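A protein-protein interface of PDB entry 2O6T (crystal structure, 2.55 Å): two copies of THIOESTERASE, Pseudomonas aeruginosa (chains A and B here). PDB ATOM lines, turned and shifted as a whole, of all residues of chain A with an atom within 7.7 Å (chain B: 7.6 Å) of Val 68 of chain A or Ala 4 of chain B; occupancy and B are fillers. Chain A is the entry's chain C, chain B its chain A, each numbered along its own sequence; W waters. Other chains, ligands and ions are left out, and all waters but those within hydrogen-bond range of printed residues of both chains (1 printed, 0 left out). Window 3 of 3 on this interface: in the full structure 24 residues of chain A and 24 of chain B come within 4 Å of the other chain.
N of Cys 72 of chain B lies within hydrogen-bond range of O of Ser 70 of chain A (2.9 Å). N of Tyr 74 of chain B lies within hydrogen-bond range of O of Val 68 of chain A (2.9 Å).
The backbone carbonyl oxygen of Tyr 74 of chain B lies within hydrogen-bond range of the backbone NH of Ala 4 of chain B (3.0 Å). The side-chain hydroxyl (OH) of Tyr 74 of chain B lies within hydrogen-bond range of the backbone carbonyl oxygen (O) of Asn 35 of chain B. The backbone carbonyl oxygen of Ala 115 of chain B sits at hydrogen-bond distance from the backbone NH of Asp 73 of chain B, at 2.7 Å. The backbone NH (N) of Leu 66 of chain A is in hydrogen-bond range of the backbone carbonyl oxygen (O) of Val 121 of chain A. N of Val 68 of chain A lies within hydrogen-bond range of O of Val 119 of chain A, 2.9 Å away. The backbone NH (N) of Val 119 of chain A lies within hydrogen-bond range of the backbone carbonyl oxygen (O) of Ser 69 of chain A, at 2.9 Å.
Among the printed residues, pairs that only touch across the chains: Val 67 of chain A with Met 3 of chain B, Ser 69 of chain A with Asp 73 of chain B, Ser 69 of chain A with Cys 72 of chain B, Val 67 of chain A with Asn 35 of chain B, Val 68 of chain A with Ala 4 of chain B, Val 67 of chain A with Tyr 74 of chain B, Val 68 of chain A with Met 3 of chain B, Val 68 of chain A with Asp 73 of chain B, Ser 69 of chain A with Tyr 74 of chain B, Ser 70 of chain A with Tyr 74 of chain B and Leu 66 of chain A with Met 3 of chain B.
Printed residues of chain B within 4 Å of Val 68 of chain A: Met 3 (3.6 Å), Ala 4 (3.5 Å), Asp 73 (3.7 Å) and Tyr 74 (2.9 Å). Of the printed residues of chain A, Asn 35 of chain B touches Val 67 (3.5 Å). Of the printed residues of chain B, Leu 66 of chain A touches Met 3 (3.9 Å). Of the printed residues of chain B, Ser 70 of chain A touches Cys 72 and Tyr 74. His 120 of chain A touches none of the printed residues of chain B. The nearest residue of chain B that does not touch Val 68 of chain A is Cys 72 of chain B (4.5 Å). The nearest residue of chain A that does not touch Ala 4 of chain B is Ser 69 of chain A (5.1 Å). The nearest printed residue of chain A that does not touch Met 3 of chain B is Val 121 of chain A (5.0 Å).
Hydrophobic or aromatic side chains of chain B that line the printed part of chain A: Met 3, Ala 4 and Tyr 74. Along chain B the printed residues that touch a printed residue of chain A span positions 3 to 74. Of the 15 printed residues of chain A, 5 touch a printed residue of chain B. Hydrophobic or aromatic side chains of chain A within 4 Å of the printed part of chain B: Leu 66, Val 67 and Val 68. Among the printed residues, no Asp or Glu carboxylate lies within 4 Å of a Lys or Arg side-chain nitrogen of the other chain.
No position is printed for both chains. Of the 13 pairs that touch across the chains among the printed residues, none has its exchanged pair printed and touching as well.
Water W1 lies within hydrogen-bond range of ND2 of Asn 35 of chain B (2.5 Å), OG of Ser 70 of chain A (2.6 Å) and OH of Tyr 74 of chain B (3.0 Å).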
ATOM      1  N   GLY A  65       2.862  28.016 -21.421  1.00  0.00           N
ATOM      2  CA  GLY A  65       3.025  27.185 -22.591  1.00  0.00           C
ATOM      3  C   GLY A  65       4.510  27.120 -22.855  1.00  0.00           C
ATOM      4  O   GLY A  65       5.145  28.180 -22.976  1.00  0.00           O
ATOM      5  N   LEU A  66       5.063  25.893 -22.896  1.00  0.00           N
ATOM      6  CA  LEU A  66       6.417  25.628 -23.391  1.00  0.00           C
ATOM      7  C   LEU A  66       6.428  24.979 -24.800  1.00  0.00           C
ATOM      8  O   LEU A  66       5.685  24.092 -25.054  1.00  0.00           O
ATOM      9  CB  LEU A  66       7.138  24.745 -22.384  1.00  0.00           C
ATOM     10  CG  LEU A  66       7.293  25.404 -21.011  1.00  0.00           C
ATOM     11  CD1 LEU A  66       8.068  24.489 -20.134  1.00  0.00           C
ATOM     12  CD2 LEU A  66       8.004  26.788 -21.118  1.00  0.00           C
ATOM     13  N   VAL A  67       7.236  25.472 -25.724  1.00  0.00           N
ATOM     14  CA  VAL A  67       7.395  24.877 -27.060  1.00  0.00           C
ATOM     15  C   VAL A  67       8.109  23.528 -26.931  1.00  0.00           C
ATOM     16  O   VAL A  67       9.294  23.447 -26.514  1.00  0.00           O
ATOM     17  CB  VAL A  67       8.146  25.880 -28.021  1.00  0.00           C
ATOM     18  CG1 VAL A  67       8.279  25.367 -29.454  1.00  0.00           C
ATOM     19  CG2 VAL A  67       7.410  27.172 -28.090  1.00  0.00           C
ATOM     20  N   VAL A  68       7.405  22.440 -27.222  1.00  0.00           N
ATOM     21  CA  VAL A  68       8.087  21.166 -27.219  1.00  0.00           C
ATOM     22  C   VAL A  68       8.614  20.803 -28.594  1.00  0.00           C
ATOM     23  O   VAL A  68       9.503  19.979 -28.714  1.00  0.00           O
ATOM     24  CB  VAL A  68       7.259  20.046 -26.646  1.00  0.00           C
ATOM     25  CG1 VAL A  68       6.820  20.423 -25.251  1.00  0.00           C
ATOM     26  CG2 VAL A  68       6.095  19.605 -27.554  1.00  0.00           C
ATOM     27  N   SER A  69       8.070  21.410 -29.641  1.00  0.00           N
ATOM     28  CA  SER A  69       8.615  21.194 -30.961  1.00  0.00           C
ATOM     29  C   SER A  69       8.072  22.168 -31.991  1.00  0.00           C
ATOM     30  O   SER A  69       7.099  22.882 -31.706  1.00  0.00           O
ATOM     31  CB  SER A  69       8.414  19.732 -31.397  1.00  0.00           C
ATOM     32  OG  SER A  69       7.128  19.569 -31.901  1.00  0.00           O
ATOM     33  N   SER A  70       8.708  22.227 -33.166  1.00  0.00           N
ATOM     34  CA  SER A  70       8.308  23.168 -34.243  1.00  0.00           C
ATOM     35  C   SER A  70       8.969  22.844 -35.559  1.00  0.00           C
ATOM     36  O   SER A  70       9.979  22.121 -35.609  1.00  0.00           O
ATOM     37  CB  SER A  70       8.695  24.618 -33.886  1.00  0.00           C
ATOM     38  OG  SER A  70      10.119  24.723 -33.778  1.00  0.00           O
ATOM     39  N   SER A  96      -3.280  18.346 -22.535  1.00  0.00           N
ATOM     40  CA  SER A  96      -2.269  19.284 -22.023  1.00  0.00           C
ATOM     41  C   SER A  96      -1.274  19.865 -23.063  1.00  0.00           C
ATOM     42  O   SER A  96      -0.233  20.416 -22.696  1.00  0.00           O
ATOM     43  CB  SER A  96      -1.502  18.628 -20.890  1.00  0.00           C
ATOM     44  OG  SER A  96      -0.979  17.398 -21.363  1.00  0.00           O
ATOM     45  N   SER A  97      -1.633  19.780 -24.340  1.00  0.00           N
ATOM     46  CA  SER A  97      -0.842  20.313 -25.410  1.00  0.00           C
ATOM     47  C   SER A  97      -1.730  20.690 -26.558  1.00  0.00           C
ATOM     48  O   SER A  97      -2.883  20.260 -26.644  1.00  0.00           O
ATOM     49  CB  SER A  97       0.120  19.265 -25.921  1.00  0.00           C
ATOM     50  OG  SER A  97      -0.581  18.152 -26.403  1.00  0.00           O
ATOM     51  N   VAL A  98      -1.166  21.455 -27.483  1.00  0.00           N
ATOM     52  CA  VAL A  98      -1.916  21.890 -28.645  1.00  0.00           C
ATOM     53  C   VAL A  98      -0.955  22.070 -29.799  1.00  0.00           C
ATOM     54  O   VAL A  98       0.157  22.497 -29.566  1.00  0.00           O
ATOM     55  CB  VAL A  98      -2.640  23.176 -28.339  1.00  0.00           C
ATOM     56  CG1 VAL A  98      -1.640  24.232 -27.837  1.00  0.00           C
ATOM     57  CG2 VAL A  98      -3.438  23.645 -29.551  1.00  0.00           C
ATOM     58  N   PHE A 118       3.824  24.606 -34.698  1.00  0.00           N
ATOM     59  CA  PHE A 118       4.472  24.337 -33.454  1.00  0.00           C
ATOM     60  C   PHE A 118       3.614  23.862 -32.315  1.00  0.00           C
ATOM     61  O   PHE A 118       2.414  23.952 -32.366  1.00  0.00           O
ATOM     62  CB  PHE A 118       5.423  25.430 -33.110  1.00  0.00           C
ATOM     63  CG  PHE A 118       4.876  26.547 -32.270  1.00  0.00           C
ATOM     64  CD1 PHE A 118       4.906  27.808 -32.734  1.00  0.00           C
ATOM     65  CD2 PHE A 118       4.530  26.345 -30.921  1.00  0.00           C
ATOM     66  CE1 PHE A 118       4.489  28.865 -31.921  1.00  0.00           C
ATOM     67  CE2 PHE A 118       4.116  27.424 -30.106  1.00  0.00           C
ATOM     68  CZ  PHE A 118       4.110  28.669 -30.615  1.00  0.00           C
ATOM     69  N   VAL A 119       4.240  23.265 -31.320  1.00  0.00           N
ATOM     70  CA  VAL A 119       3.483  22.553 -30.300  1.00  0.00           C
ATOM     71  C   VAL A 119       3.774  23.118 -28.904  1.00  0.00           C
ATOM     72  O   VAL A 119       4.952  23.235 -28.490  1.00  0.00           O
ATOM     73  CB  VAL A 119       3.790  21.034 -30.338  1.00  0.00           C
ATOM     74  CG1 VAL A 119       2.900  20.265 -29.334  1.00  0.00           C
ATOM     75  CG2 VAL A 119       3.607  20.497 -31.751  1.00  0.00           C
ATOM     76  N   HIS A 120       2.714  23.469 -28.194  1.00  0.00           N
ATOM     77  CA  HIS A 120       2.848  23.876 -26.831  1.00  0.00           C
ATOM     78  C   HIS A 120       2.472  22.747 -25.911  1.00  0.00           C
ATOM     79  O   HIS A 120       1.470  22.021 -26.159  1.00  0.00           O
ATOM     80  CB  HIS A 120       1.876  24.975 -26.547  1.00  0.00           C
ATOM     81  CG  HIS A 120       2.460  26.323 -26.568  1.00  0.00           C
ATOM     82  ND1 HIS A 120       1.676  27.454 -26.619  1.00  0.00           N
ATOM     83  CD2 HIS A 120       3.744  26.745 -26.504  1.00  0.00           C
ATOM     84  CE1 HIS A 120       2.453  28.517 -26.600  1.00  0.00           C
ATOM     85  NE2 HIS A 120       3.713  28.115 -26.546  1.00  0.00           N
ATOM     86  N   VAL A 121       3.229  22.617 -24.822  1.00  0.00           N
ATOM     87  CA  VAL A 121       2.722  21.870 -23.663  1.00  0.00           C
ATOM     88  C   VAL A 121       2.527  22.884 -22.547  1.00  0.00           C
ATOM     89  O   VAL A 121       3.281  23.863 -22.435  1.00  0.00           O
ATOM     90  CB  VAL A 121       3.644  20.681 -23.183  1.00  0.00           C
ATOM     91  CG1 VAL A 121       3.076  20.057 -21.917  1.00  0.00           C
ATOM     92  CG2 VAL A 121       3.727  19.583 -24.236  1.00  0.00           C
ATOM     93  N   PHE A 122       1.492  22.659 -21.746  1.00  0.00           N
ATOM     94  CA  PHE A 122       1.155  23.555 -20.666  1.00  0.00           C
ATOM     95  C   PHE A 122       1.581  23.005 -19.333  1.00  0.00           C
ATOM     96  O   PHE A 122       1.206  21.882 -18.925  1.00  0.00           O
ATOM     97  CB  PHE A 122      -0.318  23.904 -20.722  1.00  0.00           C
ATOM     98  CG  PHE A 122      -0.638  24.798 -21.870  1.00  0.00           C
ATOM     99  CD1 PHE A 122      -0.996  24.255 -23.099  1.00  0.00           C
ATOM    100  CD2 PHE A 122      -0.499  26.188 -21.742  1.00  0.00           C
ATOM    101  CE1 PHE A 122      -1.265  25.081 -24.172  1.00  0.00           C
ATOM    102  CE2 PHE A 122      -0.754  27.038 -22.796  1.00  0.00           C
ATOM    103  CZ  PHE A 122      -1.132  26.495 -24.021  1.00  0.00           C
ATOM    104  N   VAL A 123       2.399  23.799 -18.657  1.00  0.00           N
ATOM    105  CA  VAL A 123       3.008  23.333 -17.445  1.00  0.00           C
ATOM    106  C   VAL A 123       2.784  24.314 -16.310  1.00  0.00           C
ATOM    107  O   VAL A 123       2.432  25.498 -16.508  1.00  0.00           O
ATOM    108  CB  VAL A 123       4.546  23.035 -17.641  1.00  0.00           C
ATOM    109  CG1 VAL A 123       4.774  22.109 -18.849  1.00  0.00           C
ATOM    110  CG2 VAL A 123       5.354  24.312 -17.811  1.00  0.00           C
ATOM    111  N   HIS B   2       8.374  17.910 -18.228  1.00  0.00           N
ATOM    112  CA  HIS B   2       9.125  17.356 -19.422  1.00  0.00           C
ATOM    113  C   HIS B   2       8.463  17.798 -20.761  1.00  0.00           C
ATOM    114  O   HIS B   2       7.454  18.533 -20.751  1.00  0.00           O
ATOM    115  CB  HIS B   2       9.332  15.825 -19.316  1.00  0.00           C
ATOM    116  CG  HIS B   2      10.710  15.424 -18.847  1.00  0.00           C
ATOM    117  N   MET B   3       9.034  17.399 -21.894  1.00  0.00           N
ATOM    118  CA  MET B   3       8.700  18.054 -23.146  1.00  0.00           C
ATOM    119  C   MET B   3       8.464  17.053 -24.318  1.00  0.00           C
ATOM    120  O   MET B   3       7.502  16.282 -24.293  1.00  0.00           O
ATOM    121  CB  MET B   3       9.742  19.172 -23.485  1.00  0.00           C
ATOM    122  CG  MET B   3      10.155  20.120 -22.317  1.00  0.00           C
ATOM    123  SD  MET B   3      11.360  21.466 -22.700  1.00  0.00           S
ATOM    124  CE  MET B   3      10.304  22.690 -23.487  1.00  0.00           C
ATOM    125  N   ALA B   4       9.311  17.096 -25.339  1.00  0.00           N
ATOM    126  CA  ALA B   4       9.113  16.330 -26.536  1.00  0.00           C
ATOM    127  C   ALA B   4       9.331  14.904 -26.167  1.00  0.00           C
ATOM    128  O   ALA B   4      10.149  14.611 -25.280  1.00  0.00           O
ATOM    129  CB  ALA B   4      10.089  16.746 -27.622  1.00  0.00           C
ATOM    130  N   THR B   5       8.598  14.020 -26.828  1.00  0.00           N
ATOM    131  CA  THR B   5       8.597  12.626 -26.438  1.00  0.00           C
ATOM    132  C   THR B   5       9.340  11.765 -27.453  1.00  0.00           C
ATOM    133  O   THR B   5       9.478  10.560 -27.261  1.00  0.00           O
ATOM    134  CB  THR B   5       7.137  12.076 -26.104  1.00  0.00           C
ATOM    135  OG1 THR B   5       6.235  12.264 -27.211  1.00  0.00           O
ATOM    136  CG2 THR B   5       6.568  12.769 -24.874  1.00  0.00           C
ATOM    137  N   ALA B   6       9.810  12.390 -28.529  1.00  0.00           N
ATOM    138  CA  ALA B   6      10.728  11.771 -29.481  1.00  0.00           C
ATOM    139  C   ALA B   6      11.941  11.224 -28.724  1.00  0.00           C
ATOM    140  O   ALA B   6      12.292  11.773 -27.693  1.00  0.00           O
ATOM    141  CB  ALA B   6      11.157  12.806 -30.512  1.00  0.00           C
ATOM    142  N   PRO B   7      12.588  10.141 -29.221  1.00  0.00           N
ATOM    143  CA  PRO B   7      13.705   9.541 -28.452  1.00  0.00           C
ATOM    144  C   PRO B   7      14.916  10.463 -28.505  1.00  0.00           C
ATOM    145  O   PRO B   7      15.165  11.068 -29.544  1.00  0.00           O
ATOM    146  CB  PRO B   7      14.024   8.258 -29.213  1.00  0.00           C
ATOM    147  CG  PRO B   7      12.999   8.119 -30.280  1.00  0.00           C
ATOM    148  CD  PRO B   7      12.391   9.459 -30.515  1.00  0.00           C
ATOM    149  N   ARG B   8      15.644  10.602 -27.402  1.00  0.00           N
ATOM    150  CA  ARG B   8      16.741  11.571 -27.408  1.00  0.00           C
ATOM    151  C   ARG B   8      17.948  10.990 -28.094  1.00  0.00           C
ATOM    152  O   ARG B   8      18.354   9.875 -27.795  1.00  0.00           O
ATOM    153  CB  ARG B   8      17.119  12.041 -26.013  1.00  0.00           C
ATOM    154  CG  ARG B   8      15.962  12.583 -25.274  1.00  0.00           C
ATOM    155  CD  ARG B   8      16.281  12.741 -23.830  1.00  0.00           C
ATOM    156  NE  ARG B   8      17.102  13.920 -23.556  1.00  0.00           N
ATOM    157  CZ  ARG B   8      17.051  14.588 -22.401  1.00  0.00           C
ATOM    158  NH1 ARG B   8      17.847  15.632 -22.216  1.00  0.00           N
ATOM    159  NH2 ARG B   8      16.207  14.201 -21.419  1.00  0.00           N
ATOM    160  N   ASN B  35      13.065  28.973 -27.592  1.00  0.00           N
ATOM    161  CA  ASN B  35      13.116  27.931 -28.614  1.00  0.00           C
ATOM    162  C   ASN B  35      13.681  28.461 -29.925  1.00  0.00           C
ATOM    163  O   ASN B  35      14.370  27.739 -30.634  1.00  0.00           O
ATOM    164  CB  ASN B  35      11.724  27.332 -28.854  1.00  0.00           C
ATOM    165  CG  ASN B  35      10.673  28.399 -29.228  1.00  0.00           C
ATOM    166  OD1 ASN B  35      10.208  29.176 -28.375  1.00  0.00           O
ATOM    167  ND2 ASN B  35      10.325  28.456 -30.500  1.00  0.00           N
ATOM    168  N   CYS B  72      12.704  21.152 -35.164  1.00  0.00           N
ATOM    169  CA  CYS B  72      13.455  20.900 -33.931  1.00  0.00           C
ATOM    170  C   CYS B  72      12.537  20.312 -32.867  1.00  0.00           C
ATOM    171  O   CYS B  72      11.361  20.698 -32.766  1.00  0.00           O
ATOM    172  CB  CYS B  72      14.012  22.254 -33.439  1.00  0.00           C
ATOM    173  SG  CYS B  72      15.055  22.147 -31.996  1.00  0.00           S
ATOM    174  N   ASP B  73      13.071  19.402 -32.058  1.00  0.00           N
ATOM    175  CA  ASP B  73      12.328  18.863 -30.897  1.00  0.00           C
ATOM    176  C   ASP B  73      13.094  19.276 -29.692  1.00  0.00           C
ATOM    177  O   ASP B  73      14.341  19.184 -29.706  1.00  0.00           O
ATOM    178  CB  ASP B  73      12.281  17.324 -30.903  1.00  0.00           C
ATOM    179  CG  ASP B  73      11.342  16.753 -31.975  1.00  0.00           C
ATOM    180  OD1 ASP B  73      10.516  17.464 -32.598  1.00  0.00           O
ATOM    181  OD2 ASP B  73      11.418  15.550 -32.199  1.00  0.00           O
ATOM    182  N   TYR B  74      12.371  19.672 -28.634  1.00  0.00           N
ATOM    183  CA  TYR B  74      13.020  20.123 -27.418  1.00  0.00           C
ATOM    184  C   TYR B  74      12.810  19.168 -26.270  1.00  0.00           C
ATOM    185  O   TYR B  74      11.638  18.878 -25.899  1.00  0.00           O
ATOM    186  CB  TYR B  74      12.514  21.497 -27.035  1.00  0.00           C
ATOM    187  CG  TYR B  74      12.624  22.491 -28.159  1.00  0.00           C
ATOM    188  CD1 TYR B  74      11.620  22.595 -29.140  1.00  0.00           C
ATOM    189  CD2 TYR B  74      13.744  23.337 -28.252  1.00  0.00           C
ATOM    190  CE1 TYR B  74      11.749  23.502 -30.168  1.00  0.00           C
ATOM    191  CE2 TYR B  74      13.872  24.247 -29.274  1.00  0.00           C
ATOM    192  CZ  TYR B  74      12.875  24.324 -30.222  1.00  0.00           C
ATOM    193  OH  TYR B  74      13.005  25.280 -31.210  1.00  0.00           O
ATOM    194  N   PHE B  75      13.921  18.717 -25.673  1.00  0.00           N
ATOM    195  CA  PHE B  75      13.832  17.686 -24.614  1.00  0.00           C
ATOM    196  C   PHE B  75      14.022  18.194 -23.191  1.00  0.00           C
ATOM    197  O   PHE B  75      13.424  17.650 -22.276  1.00  0.00           O
ATOM    198  CB  PHE B  75      14.804  16.497 -24.835  1.00  0.00           C
ATOM    199  CG  PHE B  75      14.810  15.987 -26.216  1.00  0.00           C
ATOM    200  CD1 PHE B  75      15.747  16.450 -27.129  1.00  0.00           C
ATOM    201  CD2 PHE B  75      13.840  15.071 -26.638  1.00  0.00           C
ATOM    202  CE1 PHE B  75      15.749  15.976 -28.449  1.00  0.00           C
ATOM    203  CE2 PHE B  75      13.840  14.597 -27.961  1.00  0.00           C
ATOM    204  CZ  PHE B  75      14.811  15.053 -28.857  1.00  0.00           C
ATOM    205  N   ALA B  76      14.895  19.171 -23.004  1.00  0.00           N
ATOM    206  CA  ALA B  76      15.219  19.685 -21.670  1.00  0.00           C
ATOM    207  C   ALA B  76      15.794  21.052 -21.883  1.00  0.00           C
ATOM    208  O   ALA B  76      16.541  21.256 -22.832  1.00  0.00           O
ATOM    209  CB  ALA B  76      16.239  18.789 -20.941  1.00  0.00           C
ATOM    210  N   CYS B 113      19.780  18.087 -25.455  1.00  0.00           N
ATOM    211  CA  CYS B 113      18.766  18.885 -24.818  1.00  0.00           C
ATOM    212  C   CYS B 113      17.717  19.294 -25.846  1.00  0.00           C
ATOM    213  O   CYS B 113      16.572  19.614 -25.486  1.00  0.00           O
ATOM    214  CB  CYS B 113      19.402  20.117 -24.202  1.00  0.00           C
ATOM    215  SG  CYS B 113      20.519  19.726 -22.862  1.00  0.00           S
ATOM    216  N   ALA B 115      17.163  18.624 -30.469  1.00  0.00           N
ATOM    217  CA  ALA B 115      17.686  18.098 -31.705  1.00  0.00           C
ATOM    218  C   ALA B 115      16.734  18.449 -32.851  1.00  0.00           C
ATOM    219  O   ALA B 115      15.508  18.400 -32.691  1.00  0.00           O
ATOM    220  CB  ALA B 115      17.892  16.595 -31.605  1.00  0.00           C
HETATM  221  O   HOH W   1      10.738  26.853 -32.342  1.00  0.00           O
